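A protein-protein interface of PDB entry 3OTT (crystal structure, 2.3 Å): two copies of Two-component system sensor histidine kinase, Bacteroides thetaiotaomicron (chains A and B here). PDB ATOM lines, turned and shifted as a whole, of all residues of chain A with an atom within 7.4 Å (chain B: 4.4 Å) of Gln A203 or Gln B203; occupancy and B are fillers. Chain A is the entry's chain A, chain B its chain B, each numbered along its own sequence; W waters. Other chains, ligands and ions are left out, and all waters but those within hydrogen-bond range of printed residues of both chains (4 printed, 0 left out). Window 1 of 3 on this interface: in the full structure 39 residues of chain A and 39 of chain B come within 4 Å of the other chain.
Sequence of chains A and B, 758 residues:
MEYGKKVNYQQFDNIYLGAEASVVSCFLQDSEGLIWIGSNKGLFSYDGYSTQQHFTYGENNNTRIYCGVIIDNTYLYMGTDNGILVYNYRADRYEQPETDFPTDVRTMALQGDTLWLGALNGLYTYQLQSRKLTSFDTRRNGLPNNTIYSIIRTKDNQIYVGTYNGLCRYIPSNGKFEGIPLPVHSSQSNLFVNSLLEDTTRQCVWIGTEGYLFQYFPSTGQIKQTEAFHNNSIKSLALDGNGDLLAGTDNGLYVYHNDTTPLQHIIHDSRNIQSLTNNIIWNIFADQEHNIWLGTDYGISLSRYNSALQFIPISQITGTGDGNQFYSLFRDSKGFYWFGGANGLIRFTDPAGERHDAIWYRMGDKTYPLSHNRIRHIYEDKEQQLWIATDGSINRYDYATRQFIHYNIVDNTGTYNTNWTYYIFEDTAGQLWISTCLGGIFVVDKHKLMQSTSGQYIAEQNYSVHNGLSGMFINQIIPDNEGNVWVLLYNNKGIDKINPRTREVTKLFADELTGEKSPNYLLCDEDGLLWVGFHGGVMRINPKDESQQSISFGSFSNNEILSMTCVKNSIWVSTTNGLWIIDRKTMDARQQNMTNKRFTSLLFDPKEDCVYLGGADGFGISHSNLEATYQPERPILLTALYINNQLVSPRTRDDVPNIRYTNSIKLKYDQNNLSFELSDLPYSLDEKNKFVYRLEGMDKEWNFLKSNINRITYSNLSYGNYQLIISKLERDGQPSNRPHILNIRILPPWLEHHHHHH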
ATOM      1  N   ASP A 156     -30.488 -25.551  12.315  1.00  0.00           N
ATOM      2  CA  ASP A 156     -31.752 -25.514  13.020  1.00  0.00           C
ATOM      3  C   ASP A 156     -32.628 -26.674  12.580  1.00  0.00           C
ATOM      4  O   ASP A 156     -33.807 -26.643  12.817  1.00  0.00           O
ATOM      5  CB  ASP A 156     -32.472 -24.176  12.775  1.00  0.00           C
ATOM      6  CG  ASP A 156     -32.932 -24.037  11.345  1.00  0.00           C
ATOM      7  OD1 ASP A 156     -32.517 -24.874  10.518  1.00  0.00           O
ATOM      8  OD2 ASP A 156     -33.730 -23.127  11.036  1.00  0.00           O
ATOM      9  N   GLU A 198     -25.281 -24.483   3.449  1.00  0.00           N
ATOM     10  CA  GLU A 198     -25.547 -23.645   4.617  1.00  0.00           C
ATOM     11  C   GLU A 198     -24.361 -22.791   4.973  1.00  0.00           C
ATOM     12  O   GLU A 198     -23.291 -23.326   5.089  1.00  0.00           O
ATOM     13  CB  GLU A 198     -25.827 -24.493   5.863  1.00  0.00           C
ATOM     14  CG  GLU A 198     -26.266 -23.595   7.049  1.00  0.00           C
ATOM     15  CD  GLU A 198     -26.721 -24.352   8.286  1.00  0.00           C
ATOM     16  OE1 GLU A 198     -26.201 -25.465   8.597  1.00  0.00           O
ATOM     17  OE2 GLU A 198     -27.597 -23.768   8.980  1.00  0.00           O
ATOM     18  N   ASP A 199     -24.570 -21.473   5.173  1.00  0.00           N
ATOM     19  CA  ASP A 199     -23.540 -20.542   5.572  1.00  0.00           C
ATOM     20  C   ASP A 199     -24.012 -19.887   6.889  1.00  0.00           C
ATOM     21  O   ASP A 199     -24.941 -19.088   6.911  1.00  0.00           O
ATOM     22  CB  ASP A 199     -23.329 -19.506   4.468  1.00  0.00           C
ATOM     23  CG  ASP A 199     -22.152 -18.559   4.736  1.00  0.00           C
ATOM     24  OD1 ASP A 199     -21.817 -18.351   5.913  1.00  0.00           O
ATOM     25  OD2 ASP A 199     -21.569 -17.987   3.758  1.00  0.00           O
ATOM     26  N   THR A 200     -23.348 -20.254   7.979  1.00  0.00           N
ATOM     27  CA  THR A 200     -23.775 -19.991   9.371  1.00  0.00           C
ATOM     28  C   THR A 200     -23.285 -18.643   9.782  1.00  0.00           C
ATOM     29  O   THR A 200     -23.812 -18.056  10.671  1.00  0.00           O
ATOM     30  CB  THR A 200     -23.068 -20.997  10.300  1.00  0.00           C
ATOM     31  OG1 THR A 200     -23.851 -22.184  10.328  1.00  0.00           O
ATOM     32  CG2 THR A 200     -23.048 -20.505  11.621  1.00  0.00           C
ATOM     33  N   THR A 201     -22.249 -18.164   9.118  1.00  0.00           N
ATOM     34  CA  THR A 201     -21.733 -16.861   9.376  1.00  0.00           C
ATOM     35  C   THR A 201     -22.610 -15.823   8.693  1.00  0.00           C
ATOM     36  O   THR A 201     -23.014 -14.881   9.337  1.00  0.00           O
ATOM     37  CB  THR A 201     -20.291 -16.763   8.859  1.00  0.00           C
ATOM     38  OG1 THR A 201     -19.544 -17.768   9.519  1.00  0.00           O
ATOM     39  CG2 THR A 201     -19.639 -15.396   9.166  1.00  0.00           C
ATOM     40  N   ARG A 202     -22.891 -15.999   7.399  1.00  0.00           N
ATOM     41  CA  ARG A 202     -23.751 -15.057   6.659  1.00  0.00           C
ATOM     42  C   ARG A 202     -25.254 -15.310   6.932  1.00  0.00           C
ATOM     43  O   ARG A 202     -26.084 -14.488   6.537  1.00  0.00           O
ATOM     44  CB  ARG A 202     -23.452 -15.125   5.146  1.00  0.00           C
ATOM     45  CG  ARG A 202     -22.068 -14.605   4.752  1.00  0.00           C
ATOM     46  CD  ARG A 202     -21.807 -14.729   3.233  1.00  0.00           C
ATOM     47  NE  ARG A 202     -20.430 -14.309   2.897  1.00  0.00           N
ATOM     48  CZ  ARG A 202     -19.358 -15.108   2.903  1.00  0.00           C
ATOM     49  NH1 ARG A 202     -19.475 -16.429   3.132  1.00  0.00           N
ATOM     50  NH2 ARG A 202     -18.174 -14.596   2.617  1.00  0.00           N
ATOM     51  N   GLN A 203     -25.567 -16.421   7.617  1.00  0.00           N
ATOM     52  CA  GLN A 203     -26.949 -16.862   7.977  1.00  0.00           C
ATOM     53  C   GLN A 203     -27.796 -17.136   6.755  1.00  0.00           C
ATOM     54  O   GLN A 203     -28.950 -16.711   6.652  1.00  0.00           O
ATOM     55  CB  GLN A 203     -27.643 -15.917   9.005  1.00  0.00           C
ATOM     56  CG  GLN A 203     -26.832 -15.759  10.252  1.00  0.00           C
ATOM     57  CD  GLN A 203     -27.454 -14.923  11.334  1.00  0.00           C
ATOM     58  OE1 GLN A 203     -27.771 -13.752  11.148  1.00  0.00           O
ATOM     59  NE2 GLN A 203     -27.544 -15.500  12.507  1.00  0.00           N
ATOM     60  N   CYS A 204     -27.225 -17.863   5.809  1.00  0.00           N
ATOM     61  CA  CYS A 204     -27.963 -18.111   4.563  1.00  0.00           C
ATOM     62  C   CYS A 204     -27.775 -19.526   4.089  1.00  0.00           C
ATOM     63  O   CYS A 204     -26.889 -20.248   4.572  1.00  0.00           O
ATOM     64  CB  CYS A 204     -27.585 -17.135   3.451  1.00  0.00           C
ATOM     65  SG  CYS A 204     -25.880 -17.237   2.830  1.00  0.00           S
ATOM     66  N   VAL A 205     -28.631 -19.910   3.153  1.00  0.00           N
ATOM     67  CA  VAL A 205     -28.375 -21.039   2.291  1.00  0.00           C
ATOM     68  C   VAL A 205     -28.022 -20.505   0.902  1.00  0.00           C
ATOM     69  O   VAL A 205     -28.848 -19.787   0.276  1.00  0.00           O
ATOM     70  CB  VAL A 205     -29.657 -21.853   2.234  1.00  0.00           C
ATOM     71  CG1 VAL A 205     -29.581 -22.988   1.139  1.00  0.00           C
ATOM     72  CG2 VAL A 205     -29.949 -22.392   3.659  1.00  0.00           C
ATOM     73  N   TRP A 206     -26.809 -20.829   0.436  1.00  0.00           N
ATOM     74  CA  TRP A 206     -26.337 -20.585  -0.944  1.00  0.00           C
ATOM     75  C   TRP A 206     -26.961 -21.621  -1.927  1.00  0.00           C
ATOM     76  O   TRP A 206     -27.006 -22.824  -1.647  1.00  0.00           O
ATOM     77  CB  TRP A 206     -24.826 -20.728  -0.997  1.00  0.00           C
ATOM     78  CG  TRP A 206     -24.053 -19.630  -0.315  1.00  0.00           C
ATOM     79  CD1 TRP A 206     -23.547 -19.653   0.929  1.00  0.00           C
ATOM     80  CD2 TRP A 206     -23.737 -18.310  -0.859  1.00  0.00           C
ATOM     81  NE1 TRP A 206     -22.906 -18.470   1.203  1.00  0.00           N
ATOM     82  CE2 TRP A 206     -22.995 -17.628   0.128  1.00  0.00           C
ATOM     83  CE3 TRP A 206     -23.942 -17.695  -2.099  1.00  0.00           C
ATOM     84  CZ2 TRP A 206     -22.460 -16.357  -0.073  1.00  0.00           C
ATOM     85  CZ3 TRP A 206     -23.435 -16.426  -2.307  1.00  0.00           C
ATOM     86  CH2 TRP A 206     -22.712 -15.748  -1.281  1.00  0.00           C
ATOM     87  N   GLN A 215     -28.580 -16.237  -2.578  1.00  0.00           N
ATOM     88  CA  GLN A 215     -28.632 -16.477  -1.166  1.00  0.00           C
ATOM     89  C   GLN A 215     -30.069 -16.412  -0.644  1.00  0.00           C
ATOM     90  O   GLN A 215     -30.767 -15.417  -0.877  1.00  0.00           O
ATOM     91  CB  GLN A 215     -27.758 -15.466  -0.403  1.00  0.00           C
ATOM     92  CG  GLN A 215     -26.259 -15.507  -0.707  1.00  0.00           C
ATOM     93  CD  GLN A 215     -25.566 -14.257  -0.160  1.00  0.00           C
ATOM     94  OE1 GLN A 215     -25.262 -14.172   1.035  1.00  0.00           O
ATOM     95  NE2 GLN A 215     -25.319 -13.282  -1.030  1.00  0.00           N
ATOM     96  N   TYR A 216     -30.510 -17.478   0.032  1.00  0.00           N
ATOM     97  CA  TYR A 216     -31.778 -17.518   0.710  1.00  0.00           C
ATOM     98  C   TYR A 216     -31.566 -17.277   2.239  1.00  0.00           C
ATOM     99  O   TYR A 216     -30.809 -18.002   2.934  1.00  0.00           O
ATOM    100  CB  TYR A 216     -32.487 -18.837   0.407  1.00  0.00           C
ATOM    101  CG  TYR A 216     -33.781 -19.026   1.194  1.00  0.00           C
ATOM    102  CD1 TYR A 216     -34.910 -18.273   0.906  1.00  0.00           C
ATOM    103  CD2 TYR A 216     -33.858 -19.952   2.236  1.00  0.00           C
ATOM    104  CE1 TYR A 216     -36.094 -18.401   1.673  1.00  0.00           C
ATOM    105  CE2 TYR A 216     -35.027 -20.112   2.993  1.00  0.00           C
ATOM    106  CZ  TYR A 216     -36.127 -19.331   2.714  1.00  0.00           C
ATOM    107  OH  TYR A 216     -37.269 -19.500   3.447  1.00  0.00           O
ATOM    108  N   PHE A 217     -32.204 -16.235   2.758  1.00  0.00           N
ATOM    109  CA  PHE A 217     -32.176 -15.927   4.195  1.00  0.00           C
ATOM    110  C   PHE A 217     -33.491 -16.429   4.849  1.00  0.00           C
ATOM    111  O   PHE A 217     -34.509 -15.793   4.705  1.00  0.00           O
ATOM    112  CB  PHE A 217     -32.021 -14.426   4.364  1.00  0.00           C
ATOM    113  CG  PHE A 217     -30.757 -13.907   3.786  1.00  0.00           C
ATOM    114  CD1 PHE A 217     -30.715 -13.384   2.469  1.00  0.00           C
ATOM    115  CD2 PHE A 217     -29.575 -13.958   4.516  1.00  0.00           C
ATOM    116  CE1 PHE A 217     -29.518 -12.913   1.907  1.00  0.00           C
ATOM    117  CE2 PHE A 217     -28.402 -13.506   3.965  1.00  0.00           C
ATOM    118  CZ  PHE A 217     -28.370 -12.975   2.640  1.00  0.00           C
ATOM    119  N   PRO A 218     -33.488 -17.618   5.501  1.00  0.00           N
ATOM    120  CA  PRO A 218     -34.707 -18.177   6.180  1.00  0.00           C
ATOM    121  C   PRO A 218     -35.249 -17.204   7.247  1.00  0.00           C
ATOM    122  O   PRO A 218     -36.435 -17.228   7.573  1.00  0.00           O
ATOM    123  CB  PRO A 218     -34.184 -19.446   6.952  1.00  0.00           C
ATOM    124  CG  PRO A 218     -32.814 -19.709   6.407  1.00  0.00           C
ATOM    125  CD  PRO A 218     -32.282 -18.437   5.710  1.00  0.00           C
ATOM    126  N   SER A 219     -34.396 -16.366   7.820  1.00  0.00           N
ATOM    127  CA  SER A 219     -34.911 -15.368   8.752  1.00  0.00           C
ATOM    128  C   SER A 219     -36.028 -14.482   8.172  1.00  0.00           C
ATOM    129  O   SER A 219     -37.013 -14.233   8.886  1.00  0.00           O
ATOM    130  CB  SER A 219     -33.814 -14.501   9.346  1.00  0.00           C
ATOM    131  OG  SER A 219     -33.032 -13.901   8.326  1.00  0.00           O
ATOM    132  N   THR A 220     -35.867 -13.994   6.938  1.00  0.00           N
ATOM    133  CA  THR A 220     -36.863 -13.107   6.325  1.00  0.00           C
ATOM    134  C   THR A 220     -37.556 -13.713   5.089  1.00  0.00           C
ATOM    135  O   THR A 220     -38.486 -13.120   4.565  1.00  0.00           O
ATOM    136  CB  THR A 220     -36.224 -11.728   5.921  1.00  0.00           C
ATOM    137  OG1 THR A 220     -35.197 -11.944   4.904  1.00  0.00           O
ATOM    138  CG2 THR A 220     -35.567 -11.026   7.193  1.00  0.00           C
ATOM    139  N   ASP B 199     -32.236 -12.763  19.452  1.00  0.00           N
ATOM    140  CA  ASP B 199     -33.089 -13.938  19.245  1.00  0.00           C
ATOM    141  C   ASP B 199     -32.418 -14.804  18.180  1.00  0.00           C
ATOM    142  O   ASP B 199     -32.574 -14.527  16.996  1.00  0.00           O
ATOM    143  CB  ASP B 199     -34.452 -13.456  18.694  1.00  0.00           C
ATOM    144  CG  ASP B 199     -35.496 -14.571  18.588  1.00  0.00           C
ATOM    145  OD1 ASP B 199     -35.115 -15.751  18.562  1.00  0.00           O
ATOM    146  OD2 ASP B 199     -36.715 -14.263  18.569  1.00  0.00           O
ATOM    147  N   THR B 200     -31.711 -15.864  18.589  1.00  0.00           N
ATOM    148  CA  THR B 200     -30.956 -16.766  17.664  1.00  0.00           C
ATOM    149  C   THR B 200     -31.857 -17.652  16.812  1.00  0.00           C
ATOM    150  O   THR B 200     -31.455 -18.123  15.752  1.00  0.00           O
ATOM    151  CB  THR B 200     -29.942 -17.626  18.416  1.00  0.00           C
ATOM    152  OG1 THR B 200     -30.595 -18.294  19.505  1.00  0.00           O
ATOM    153  CG2 THR B 200     -28.891 -16.734  19.020  1.00  0.00           C
ATOM    154  N   THR B 201     -33.084 -17.881  17.252  1.00  0.00           N
ATOM    155  CA  THR B 201     -34.020 -18.699  16.487  1.00  0.00           C
ATOM    156  C   THR B 201     -34.655 -17.887  15.371  1.00  0.00           C
ATOM    157  O   THR B 201     -34.781 -18.380  14.297  1.00  0.00           O
ATOM    158  CB  THR B 201     -35.126 -19.265  17.363  1.00  0.00           C
ATOM    159  OG1 THR B 201     -34.521 -20.060  18.356  1.00  0.00           O
ATOM    160  CG2 THR B 201     -36.105 -20.167  16.539  1.00  0.00           C
ATOM    161  N   ARG B 202     -35.045 -16.640  15.608  1.00  0.00           N
ATOM    162  CA  ARG B 202     -35.502 -15.786  14.505  1.00  0.00           C
ATOM    163  C   ARG B 202     -34.337 -15.106  13.796  1.00  0.00           C
ATOM    164  O   ARG B 202     -34.531 -14.501  12.734  1.00  0.00           O
ATOM    165  CB  ARG B 202     -36.514 -14.748  14.999  1.00  0.00           C
ATOM    166  CG  ARG B 202     -37.932 -15.371  15.409  1.00  0.00           C
ATOM    167  CD  ARG B 202     -38.918 -14.341  15.997  1.00  0.00           C
ATOM    168  NE  ARG B 202     -40.079 -15.053  16.578  1.00  0.00           N
ATOM    169  CZ  ARG B 202     -40.200 -15.491  17.847  1.00  0.00           C
ATOM    170  NH1 ARG B 202     -39.260 -15.270  18.763  1.00  0.00           N
ATOM    171  NH2 ARG B 202     -41.316 -16.098  18.223  1.00  0.00           N
ATOM    172  N   GLN B 203     -33.137 -15.194  14.369  1.00  0.00           N
ATOM    173  CA  GLN B 203     -31.952 -14.494  13.824  1.00  0.00           C
ATOM    174  C   GLN B 203     -32.119 -12.974  13.658  1.00  0.00           C
ATOM    175  O   GLN B 203     -31.803 -12.415  12.579  1.00  0.00           O
ATOM    176  CB  GLN B 203     -31.487 -15.156  12.542  1.00  0.00           C
ATOM    177  CG  GLN B 203     -31.200 -16.685  12.802  1.00  0.00           C
ATOM    178  CD  GLN B 203     -30.697 -17.385  11.596  1.00  0.00           C
ATOM    179  OE1 GLN B 203     -31.269 -17.271  10.476  1.00  0.00           O
ATOM    180  NE2 GLN B 203     -29.586 -18.091  11.773  1.00  0.00           N
ATOM    181  N   CYS B 204     -32.635 -12.327  14.707  1.00  0.00           N
ATOM    182  CA  CYS B 204     -32.819 -10.884  14.715  1.00  0.00           C
ATOM    183  C   CYS B 204     -32.362 -10.337  16.048  1.00  0.00           C
ATOM    184  O   CYS B 204     -32.139 -11.059  17.013  1.00  0.00           O
ATOM    185  CB  CYS B 204     -34.315 -10.507  14.485  1.00  0.00           C
ATOM    186  SG  CYS B 204     -35.467 -11.186  15.782  1.00  0.00           S
ATOM    187  N   PHE B 217     -32.474  -7.426  11.262  1.00  0.00           N
ATOM    188  CA  PHE B 217     -31.906  -8.719  10.816  1.00  0.00           C
ATOM    189  C   PHE B 217     -30.552  -8.429  10.252  1.00  0.00           C
ATOM    190  O   PHE B 217     -30.444  -7.957   9.078  1.00  0.00           O
ATOM    191  CB  PHE B 217     -32.777  -9.364   9.715  1.00  0.00           C
ATOM    192  CG  PHE B 217     -34.174  -9.634  10.151  1.00  0.00           C
ATOM    193  CD1 PHE B 217     -34.487 -10.857  10.719  1.00  0.00           C
ATOM    194  CD2 PHE B 217     -35.190  -8.658  10.012  1.00  0.00           C
ATOM    195  CE1 PHE B 217     -35.813 -11.160  11.138  1.00  0.00           C
ATOM    196  CE2 PHE B 217     -36.493  -8.931  10.438  1.00  0.00           C
ATOM    197  CZ  PHE B 217     -36.813 -10.195  11.013  1.00  0.00           C
ATOM    198  N   PRO B 218     -29.510  -8.700  11.040  1.00  0.00           N
ATOM    199  CA  PRO B 218     -28.141  -8.339  10.635  1.00  0.00           C
ATOM    200  C   PRO B 218     -27.686  -9.053   9.364  1.00  0.00           C
ATOM    201  O   PRO B 218     -26.869  -8.511   8.625  1.00  0.00           O
ATOM    202  CB  PRO B 218     -27.253  -8.708  11.849  1.00  0.00           C
ATOM    203  CG  PRO B 218     -28.216  -9.170  12.972  1.00  0.00           C
ATOM    204  CD  PRO B 218     -29.605  -9.284  12.403  1.00  0.00           C
ATOM    205  N   SER B 219     -28.200 -10.231   9.077  1.00  0.00           N
ATOM    206  CA  SER B 219     -27.806 -10.897   7.834  1.00  0.00           C
ATOM    207  C   SER B 219     -28.163 -10.158   6.521  1.00  0.00           C
ATOM    208  O   SER B 219     -27.533 -10.401   5.511  1.00  0.00           O
ATOM    209  CB  SER B 219     -28.357 -12.295   7.787  1.00  0.00           C
ATOM    210  OG  SER B 219     -29.753 -12.191   7.707  1.00  0.00           O
HETATM  211  O   HOH W   1     -37.243 -14.764  11.542  1.00  0.00           O
HETATM  212  O   HOH W   2     -30.199 -12.068  10.404  1.00  0.00           O
HETATM  213  O   HOH W   3     -31.409 -15.808   7.948  1.00  0.00           O
HETATM  214  O   HOH W   4     -25.456 -11.857   5.631  1.00  0.00           O
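Water W3 lies within hydrogen-bond range of the side-chain hydroxyl (OG) of Ser A219, the backbone carbonyl oxygen (O) of Gln A203 and the side-chain amide oxygen (OE1) of Gln B203. Water W4 lies within hydrogen-bond range of the backbone carbonyl oxygen (O) of Ser B219 (2.5 Å) and the backbone carbonyl oxygen (O) of Arg A202 (2.9 Å). Water W1 lies within hydrogen-bond range of O of Ser A219 (2.7 Å) and O of Arg B202 (3.0 Å). Water W2 lies within hydrogen-bond range of the backbone carbonyl oxygen of Gln B203 (2.7 Å), the side-chain hydroxyl of Ser B219 (2.7 Å) and the side-chain amide oxygen of Gln A203 (3.0 Å).
Along chain A the printed residues that touch a printed residue of chain B span positions 202 to 220. Among the printed residues, 9 pairs touch across the chains. Among the printed residues, no Asp or Glu carboxylate lies within 4 Å of a Lys or Arg side-chain nitrogen of the other chain.
Arg A202 touches Ser B219 (O to CB, 3.4 Å). Ser B219 touches Gln A203. Phe A217 touches Ser B219 (CE2 to O, 3.6 Å). Arg B202 touches Ser A219 (O to CB, 3.5 Å). Ser A219 touches Gln B203. Phe B217 touches Ser A219 (CD1 to CB, 3.95 Å). OG of Ser B219 touches OG of Ser A219, 3.7 Å away. Thr A220 touches Phe B217 (CG2 to CG, 3.6 Å).
Gln B203 touches its own counterpart, Gln A203. Gln A203 touches Ser B219, and with the chains exchanged Ser A219 touches Gln B203. Phe A217 touches Ser B219, and with the chains exchanged Ser A219 touches Phe B217. Ser B219 touches its own counterpart, Ser A219. Of the 9 pairs that touch across the chains among the printed residues, 8 have their exchanged pair printed and touching as well.
The side-chain carboxylate of Asp B199 lies within salt-bridge range of the guanidinium group of Arg B202 (2.7 Å). NH1 of Arg A202 lies within salt-bridge range of OD2 of Asp A199 (2.7 Å).
The side-chain amide nitrogen (NE2) of Gln B203 sits close to the side-chain amide nitrogen (NE2) of Gln A203 (3.4 Å).
Of the printed residues of chain A, Gln B203 touches Gln A203 (3.4 Å) and Ser A219 (3.9 Å). Of the printed residues of chain A, Phe B217 touches Ser A219 and Thr A220. Of the printed residues of chain B, Phe A217 touches Ser B219. Printed residues of chain A within 4 Å of Arg B202: Ser A219. Glu A198 touches none of the printed residues of chain B. Val A205 touches none of the printed residues of chain B. The nearest printed residue of chain B that does not touch Gln A203 is Pro B218 (5.0 Å). The nearest residue of chain A that does not touch Gln B203 is Pro A218 (5.0 Å). The nearest printed residue of chain A that does not touch Phe B217 is Gln A203 (6.1 Å).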
